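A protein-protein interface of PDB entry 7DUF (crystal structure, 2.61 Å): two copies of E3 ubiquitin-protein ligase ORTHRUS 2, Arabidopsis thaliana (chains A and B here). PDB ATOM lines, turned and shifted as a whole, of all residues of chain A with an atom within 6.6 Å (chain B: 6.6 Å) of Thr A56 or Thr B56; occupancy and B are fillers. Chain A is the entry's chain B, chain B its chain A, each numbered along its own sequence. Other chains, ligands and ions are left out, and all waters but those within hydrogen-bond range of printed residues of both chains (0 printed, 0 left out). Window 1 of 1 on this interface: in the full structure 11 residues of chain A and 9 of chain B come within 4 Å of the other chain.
Leu A32 touches Leu B57, and with the chains exchanged Leu A57 touches Leu B32.
Leu A53 touches Thr B56, and with the chains exchanged Thr A56 touches Leu B53.
Thr B56 touches its own counterpart, Thr A56.
Leu A57 touches Thr B56, but with the chains exchanged Thr A56 does not touch Leu B57 (4.3 Å).
Of the 8 pairs that touch across the chains among the printed residues, 7 have their exchanged pair printed and touching as well.
Printed residues of chain A that touch a printed residue of chain B: Leu A32, Pro A50, Leu A53, Thr A56 and Leu A57.
Hydrophobic or aromatic side chains of chain A that line the printed part of chain B: Leu A32, Pro A50, Leu A53 and Leu A57.
Hydrophobic or aromatic side chains of chain B within 4 Å of the printed part of chain A: Leu B32, Pro B50, Leu B53 and Leu B57.
Among the printed residues, no Asp or Glu carboxylate lies within 4 Å of a Lys or Arg side-chain nitrogen of the other chain.
Leu A32 touches Leu B57 (CD1 to CD2, 3.5 Å).
CD of Pro A50 touches CD1 of Leu B53 (3.996 Å).
Leu A53 touches Pro B50.
CG2 of Thr B56 touches CD1 of Leu A53, 3.9 Å away.
Thr A56 touches Leu B53 (OG1 to CD1, 3.8 Å).
Thr B56 touches Thr A56.
CD2 of Leu A57 touches CG of Leu B32 (3.6 Å).
CG2 of Thr B56 touches CD2 of Leu A57, at 3.7 Å.
Lys A51 touches none of the printed residues of chain B.
Of the printed residues of chain B, Leu A53 touches Pro B50 and Thr B56.
Printed residues of chain B within 4 Å of Leu A57: Leu B32 and Thr B56.
Gln A58 touches none of the printed residues of chain B.
Of the printed residues of chain A, Pro B50 touches Leu A53.
Of the printed residues of chain A, Leu B53 touches Pro A50 and Thr A56.
Of the printed residues of chain A, Leu B57 touches Leu A32 (3.5 Å).
The nearest residue of chain B that does not touch Thr A56 is Leu B57 (4.3 Å).
The nearest printed residue of chain B that does not touch Leu A53 is Leu B32 (5.4 Å).
The backbone carbonyl oxygen of Thr B52 sits at hydrogen-bond distance from the side-chain hydroxyl of Thr B56, at 2.7 Å.
The side-chain hydroxyl (OG1) of Thr A56 is in hydrogen-bond range of the backbone carbonyl oxygen (O) of Thr A52 (2.7 Å).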
ATOM      1  N   LEU A  32       9.506  -4.283  11.731  1.00  0.00           N
ATOM      2  CA  LEU A  32       8.794  -3.012  11.791  1.00  0.00           C
ATOM      3  C   LEU A  32       8.650  -2.476  10.374  1.00  0.00           C
ATOM      4  O   LEU A  32       9.653  -2.200   9.709  1.00  0.00           O
ATOM      5  CB  LEU A  32       9.536  -2.015  12.687  1.00  0.00           C
ATOM      6  CG  LEU A  32       8.769  -0.836  13.288  1.00  0.00           C
ATOM      7  CD1 LEU A  32       7.626  -1.318  14.147  1.00  0.00           C
ATOM      8  CD2 LEU A  32       9.714   0.019  14.112  1.00  0.00           C
ATOM      9  N   THR A  33       7.410  -2.344   9.913  1.00  0.00           N
ATOM     10  CA  THR A  33       7.122  -1.898   8.555  1.00  0.00           C
ATOM     11  C   THR A  33       6.865  -0.397   8.547  1.00  0.00           C
ATOM     12  O   THR A  33       6.114   0.115   9.384  1.00  0.00           O
ATOM     13  CB  THR A  33       5.918  -2.644   7.979  1.00  0.00           C
ATOM     14  OG1 THR A  33       5.992  -4.027   8.347  1.00  0.00           O
ATOM     15  CG2 THR A  33       5.896  -2.530   6.460  1.00  0.00           C
ATOM     16  N   PRO A  50      12.107   3.139  17.965  1.00  0.00           N
ATOM     17  CA  PRO A  50      11.082   4.096  18.393  1.00  0.00           C
ATOM     18  C   PRO A  50      11.034   4.220  19.908  1.00  0.00           C
ATOM     19  O   PRO A  50      11.365   3.287  20.643  1.00  0.00           O
ATOM     20  CB  PRO A  50       9.784   3.499  17.838  1.00  0.00           C
ATOM     21  CG  PRO A  50      10.221   2.621  16.712  1.00  0.00           C
ATOM     22  CD  PRO A  50      11.541   2.059  17.139  1.00  0.00           C
ATOM     23  N   LYS A  51      10.614   5.398  20.374  1.00  0.00           N
ATOM     24  CA  LYS A  51      10.612   5.708  21.795  1.00  0.00           C
ATOM     25  C   LYS A  51       9.220   5.870  22.389  1.00  0.00           C
ATOM     26  O   LYS A  51       9.093   5.900  23.618  1.00  0.00           O
ATOM     27  CB  LYS A  51      11.423   6.985  22.061  1.00  0.00           C
ATOM     28  CG  LYS A  51      12.910   6.847  21.775  1.00  0.00           C
ATOM     29  N   THR A  52       8.181   5.984  21.565  1.00  0.00           N
ATOM     30  CA  THR A  52       6.812   6.113  22.047  1.00  0.00           C
ATOM     31  C   THR A  52       5.944   5.051  21.384  1.00  0.00           C
ATOM     32  O   THR A  52       6.388   4.309  20.502  1.00  0.00           O
ATOM     33  CB  THR A  52       6.243   7.512  21.773  1.00  0.00           C
ATOM     34  OG1 THR A  52       6.107   7.707  20.359  1.00  0.00           O
ATOM     35  CG2 THR A  52       7.155   8.583  22.341  1.00  0.00           C
ATOM     36  N   LEU A  53       4.684   4.986  21.818  1.00  0.00           N
ATOM     37  CA  LEU A  53       3.741   4.054  21.214  1.00  0.00           C
ATOM     38  C   LEU A  53       3.256   4.555  19.860  1.00  0.00           C
ATOM     39  O   LEU A  53       3.069   3.760  18.933  1.00  0.00           O
ATOM     40  CB  LEU A  53       2.559   3.821  22.157  1.00  0.00           C
ATOM     41  CG  LEU A  53       1.424   2.943  21.629  1.00  0.00           C
ATOM     42  CD1 LEU A  53       1.717   1.475  21.895  1.00  0.00           C
ATOM     43  CD2 LEU A  53       0.099   3.348  22.255  1.00  0.00           C
ATOM     44  N   ALA A  54       3.053   5.869  19.725  1.00  0.00           N
ATOM     45  CA  ALA A  54       2.614   6.421  18.449  1.00  0.00           C
ATOM     46  C   ALA A  54       3.682   6.258  17.376  1.00  0.00           C
ATOM     47  O   ALA A  54       3.369   5.936  16.224  1.00  0.00           O
ATOM     48  CB  ALA A  54       2.241   7.894  18.613  1.00  0.00           C
ATOM     49  N   SER A  55       4.950   6.475  17.733  1.00  0.00           N
ATOM     50  CA  SER A  55       6.039   6.288  16.782  1.00  0.00           C
ATOM     51  C   SER A  55       6.267   4.823  16.436  1.00  0.00           C
ATOM     52  O   SER A  55       6.977   4.537  15.466  1.00  0.00           O
ATOM     53  CB  SER A  55       7.330   6.898  17.330  1.00  0.00           C
ATOM     54  OG  SER A  55       7.435   6.705  18.730  1.00  0.00           O
ATOM     55  N   THR A  56       5.694   3.895  17.202  1.00  0.00           N
ATOM     56  CA  THR A  56       5.750   2.477  16.871  1.00  0.00           C
ATOM     57  C   THR A  56       4.566   2.046  16.014  1.00  0.00           C
ATOM     58  O   THR A  56       4.731   1.245  15.088  1.00  0.00           O
ATOM     59  CB  THR A  56       5.798   1.636  18.151  1.00  0.00           C
ATOM     60  OG1 THR A  56       6.882   2.078  18.976  1.00  0.00           O
ATOM     61  CG2 THR A  56       5.990   0.164  17.818  1.00  0.00           C
ATOM     62  N   LEU A  57       3.374   2.576  16.299  1.00  0.00           N
ATOM     63  CA  LEU A  57       2.185   2.184  15.549  1.00  0.00           C
ATOM     64  C   LEU A  57       2.225   2.738  14.130  1.00  0.00           C
ATOM     65  O   LEU A  57       1.949   2.018  13.163  1.00  0.00           O
ATOM     66  CB  LEU A  57       0.929   2.647  16.284  1.00  0.00           C
ATOM     67  CG  LEU A  57       0.732   1.952  17.633  1.00  0.00           C
ATOM     68  CD1 LEU A  57      -0.607   2.307  18.259  1.00  0.00           C
ATOM     69  CD2 LEU A  57       0.875   0.449  17.470  1.00  0.00           C
ATOM     70  N   GLN A  58       2.561   4.016  13.986  1.00  0.00           N
ATOM     71  CA  GLN A  58       2.825   4.627  12.685  1.00  0.00           C
ATOM     72  C   GLN A  58       4.314   4.971  12.674  1.00  0.00           C
ATOM     73  O   GLN A  58       4.732   6.022  13.161  1.00  0.00           O
ATOM     74  CB  GLN A  58       1.948   5.856  12.442  1.00  0.00           C
ATOM     75  CG  GLN A  58       2.426   6.748  11.300  1.00  0.00           C
ATOM     76  CD  GLN A  58       1.283   7.394  10.547  1.00  0.00           C
ATOM     77  OE1 GLN A  58       0.961   6.997   9.426  1.00  0.00           O
ATOM     78  NE2 GLN A  58       0.660   8.394  11.160  1.00  0.00           N
ATOM     79  N   TRP A  59       5.114   4.060  12.133  1.00  0.00           N
ATOM     80  CA  TRP A  59       6.564   4.188  12.140  1.00  0.00           C
ATOM     81  C   TRP A  59       7.048   4.676  10.784  1.00  0.00           C
ATOM     82  O   TRP A  59       6.625   4.161   9.742  1.00  0.00           O
ATOM     83  CB  TRP A  59       7.229   2.856  12.485  1.00  0.00           C
ATOM     84  CG  TRP A  59       8.724   2.921  12.500  1.00  0.00           C
ATOM     85  CD1 TRP A  59       9.507   3.613  13.377  1.00  0.00           C
ATOM     86  CD2 TRP A  59       9.620   2.268  11.593  1.00  0.00           C
ATOM     87  NE1 TRP A  59      10.834   3.430  13.075  1.00  0.00           N
ATOM     88  CE2 TRP A  59      10.931   2.607  11.984  1.00  0.00           C
ATOM     89  CE3 TRP A  59       9.441   1.424  10.493  1.00  0.00           C
ATOM     90  CZ2 TRP A  59      12.055   2.137  11.311  1.00  0.00           C
ATOM     91  CZ3 TRP A  59      10.560   0.959   9.826  1.00  0.00           C
ATOM     92  CH2 TRP A  59      11.849   1.315  10.238  1.00  0.00           C
ATOM     93  N   LEU B  32      -4.143  -0.655  16.492  1.00  0.00           N
ATOM     94  CA  LEU B  32      -3.383  -1.877  16.718  1.00  0.00           C
ATOM     95  C   LEU B  32      -4.218  -3.063  16.264  1.00  0.00           C
ATOM     96  O   LEU B  32      -5.383  -3.188  16.651  1.00  0.00           O
ATOM     97  CB  LEU B  32      -3.005  -2.035  18.196  1.00  0.00           C
ATOM     98  CG  LEU B  32      -1.515  -2.047  18.535  1.00  0.00           C
ATOM     99  CD1 LEU B  32      -1.290  -2.572  19.945  1.00  0.00           C
ATOM    100  CD2 LEU B  32      -0.741  -2.876  17.520  1.00  0.00           C
ATOM    101  N   THR B  33      -3.626  -3.927  15.445  1.00  0.00           N
ATOM    102  CA  THR B  33      -4.290  -5.133  14.974  1.00  0.00           C
ATOM    103  C   THR B  33      -3.696  -6.350  15.670  1.00  0.00           C
ATOM    104  O   THR B  33      -2.490  -6.402  15.933  1.00  0.00           O
ATOM    105  CB  THR B  33      -4.169  -5.285  13.454  1.00  0.00           C
ATOM    106  OG1 THR B  33      -2.971  -6.003  13.134  1.00  0.00           O
ATOM    107  CG2 THR B  33      -4.135  -3.919  12.782  1.00  0.00           C
ATOM    108  N   PRO B  50      -0.134  -1.830  25.410  1.00  0.00           N
ATOM    109  CA  PRO B  50       1.206  -2.425  25.488  1.00  0.00           C
ATOM    110  C   PRO B  50       2.235  -1.407  25.956  1.00  0.00           C
ATOM    111  O   PRO B  50       2.182  -0.230  25.597  1.00  0.00           O
ATOM    112  CB  PRO B  50       1.473  -2.881  24.049  1.00  0.00           C
ATOM    113  CG  PRO B  50       0.591  -2.011  23.211  1.00  0.00           C
ATOM    114  CD  PRO B  50      -0.652  -1.820  24.031  1.00  0.00           C
ATOM    115  N   LYS B  51       3.180  -1.875  26.775  1.00  0.00           N
ATOM    116  CA  LYS B  51       4.157  -1.000  27.407  1.00  0.00           C
ATOM    117  C   LYS B  51       5.586  -1.221  26.930  1.00  0.00           C
ATOM    118  O   LYS B  51       6.454  -0.400  27.243  1.00  0.00           O
ATOM    119  CB  LYS B  51       4.110  -1.162  28.934  1.00  0.00           C
ATOM    120  CG  LYS B  51       2.774  -0.786  29.558  1.00  0.00           C
ATOM    121  CD  LYS B  51       2.674  -1.228  31.015  1.00  0.00           C
ATOM    122  CE  LYS B  51       3.684  -2.316  31.361  1.00  0.00           C
ATOM    123  NZ  LYS B  51       3.275  -3.101  32.559  1.00  0.00           N
ATOM    124  N   THR B  52       5.859  -2.302  26.205  1.00  0.00           N
ATOM    125  CA  THR B  52       7.177  -2.544  25.641  1.00  0.00           C
ATOM    126  C   THR B  52       7.076  -2.607  24.124  1.00  0.00           C
ATOM    127  O   THR B  52       5.995  -2.790  23.557  1.00  0.00           O
ATOM    128  CB  THR B  52       7.798  -3.842  26.178  1.00  0.00           C
ATOM    129  OG1 THR B  52       7.162  -4.971  25.566  1.00  0.00           O
ATOM    130  CG2 THR B  52       7.637  -3.931  27.689  1.00  0.00           C
ATOM    131  N   LEU B  53       8.225  -2.447  23.467  1.00  0.00           N
ATOM    132  CA  LEU B  53       8.240  -2.449  22.008  1.00  0.00           C
ATOM    133  C   LEU B  53       7.915  -3.831  21.454  1.00  0.00           C
ATOM    134  O   LEU B  53       7.239  -3.947  20.425  1.00  0.00           O
ATOM    135  CB  LEU B  53       9.596  -1.969  21.495  1.00  0.00           C
ATOM    136  CG  LEU B  53       9.752  -1.959  19.975  1.00  0.00           C
ATOM    137  CD1 LEU B  53       9.561  -0.556  19.422  1.00  0.00           C
ATOM    138  CD2 LEU B  53      11.107  -2.517  19.585  1.00  0.00           C
ATOM    139  N   ALA B  54       8.384  -4.888  22.120  1.00  0.00           N
ATOM    140  CA  ALA B  54       8.093  -6.239  21.651  1.00  0.00           C
ATOM    141  C   ALA B  54       6.622  -6.586  21.843  1.00  0.00           C
ATOM    142  O   ALA B  54       6.022  -7.257  20.995  1.00  0.00           O
ATOM    143  CB  ALA B  54       8.981  -7.251  22.373  1.00  0.00           C
ATOM    144  N   SER B  55       6.023  -6.142  22.952  1.00  0.00           N
ATOM    145  CA  SER B  55       4.605  -6.401  23.176  1.00  0.00           C
ATOM    146  C   SER B  55       3.736  -5.663  22.168  1.00  0.00           C
ATOM    147  O   SER B  55       2.613  -6.093  21.887  1.00  0.00           O
ATOM    148  CB  SER B  55       4.213  -6.009  24.600  1.00  0.00           C
ATOM    149  OG  SER B  55       5.267  -6.271  25.510  1.00  0.00           O
ATOM    150  N   THR B  56       4.234  -4.554  21.618  1.00  0.00           N
ATOM    151  CA  THR B  56       3.486  -3.826  20.601  1.00  0.00           C
ATOM    152  C   THR B  56       3.586  -4.495  19.236  1.00  0.00           C
ATOM    153  O   THR B  56       2.651  -4.400  18.433  1.00  0.00           O
ATOM    154  CB  THR B  56       3.985  -2.383  20.516  1.00  0.00           C
ATOM    155  OG1 THR B  56       4.118  -1.846  21.838  1.00  0.00           O
ATOM    156  CG2 THR B  56       3.009  -1.526  19.729  1.00  0.00           C
ATOM    157  N   LEU B  57       4.696  -5.183  18.962  1.00  0.00           N
ATOM    158  CA  LEU B  57       4.872  -5.837  17.671  1.00  0.00           C
ATOM    159  C   LEU B  57       4.071  -7.131  17.593  1.00  0.00           C
ATOM    160  O   LEU B  57       3.244  -7.309  16.692  1.00  0.00           O
ATOM    161  CB  LEU B  57       6.360  -6.099  17.418  1.00  0.00           C
ATOM    162  CG  LEU B  57       7.180  -4.813  17.308  1.00  0.00           C
ATOM    163  CD1 LEU B  57       8.623  -5.090  16.918  1.00  0.00           C
ATOM    164  CD2 LEU B  57       6.519  -3.877  16.315  1.00  0.00           C
ATOM    165  N   GLN B  58       4.303  -8.046  18.532  1.00  0.00           N
ATOM    166  CA  GLN B  58       3.530  -9.284  18.615  1.00  0.00           C
ATOM    167  C   GLN B  58       2.380  -9.118  19.611  1.00  0.00           C
ATOM    168  O   GLN B  58       2.229  -9.868  20.575  1.00  0.00           O
ATOM    169  CB  GLN B  58       4.436 -10.449  18.997  1.00  0.00           C
ATOM    170  N   TRP B  59       1.563  -8.098  19.358  1.00  0.00           N
ATOM    171  CA  TRP B  59       0.449  -7.785  20.240  1.00  0.00           C
ATOM    172  C   TRP B  59      -0.705  -8.750  20.016  1.00  0.00           C
ATOM    173  O   TRP B  59      -1.025  -9.110  18.879  1.00  0.00           O
ATOM    174  CB  TRP B  59      -0.030  -6.351  20.019  1.00  0.00           C
ATOM    175  CG  TRP B  59      -1.138  -5.963  20.946  1.00  0.00           C
ATOM    176  CD1 TRP B  59      -1.042  -5.740  22.288  1.00  0.00           C
ATOM    177  CD2 TRP B  59      -2.515  -5.766  20.605  1.00  0.00           C
ATOM    178  NE1 TRP B  59      -2.271  -5.410  22.803  1.00  0.00           N
ATOM    179  CE2 TRP B  59      -3.193  -5.418  21.790  1.00  0.00           C
ATOM    180  CE3 TRP B  59      -3.238  -5.845  19.412  1.00  0.00           C
ATOM    181  CZ2 TRP B  59      -4.560  -5.153  21.816  1.00  0.00           C
ATOM    182  CZ3 TRP B  59      -4.595  -5.580  19.440  1.00  0.00           C
ATOM    183  CH2 TRP B  59      -5.240  -5.236  20.634  1.00  0.00           C
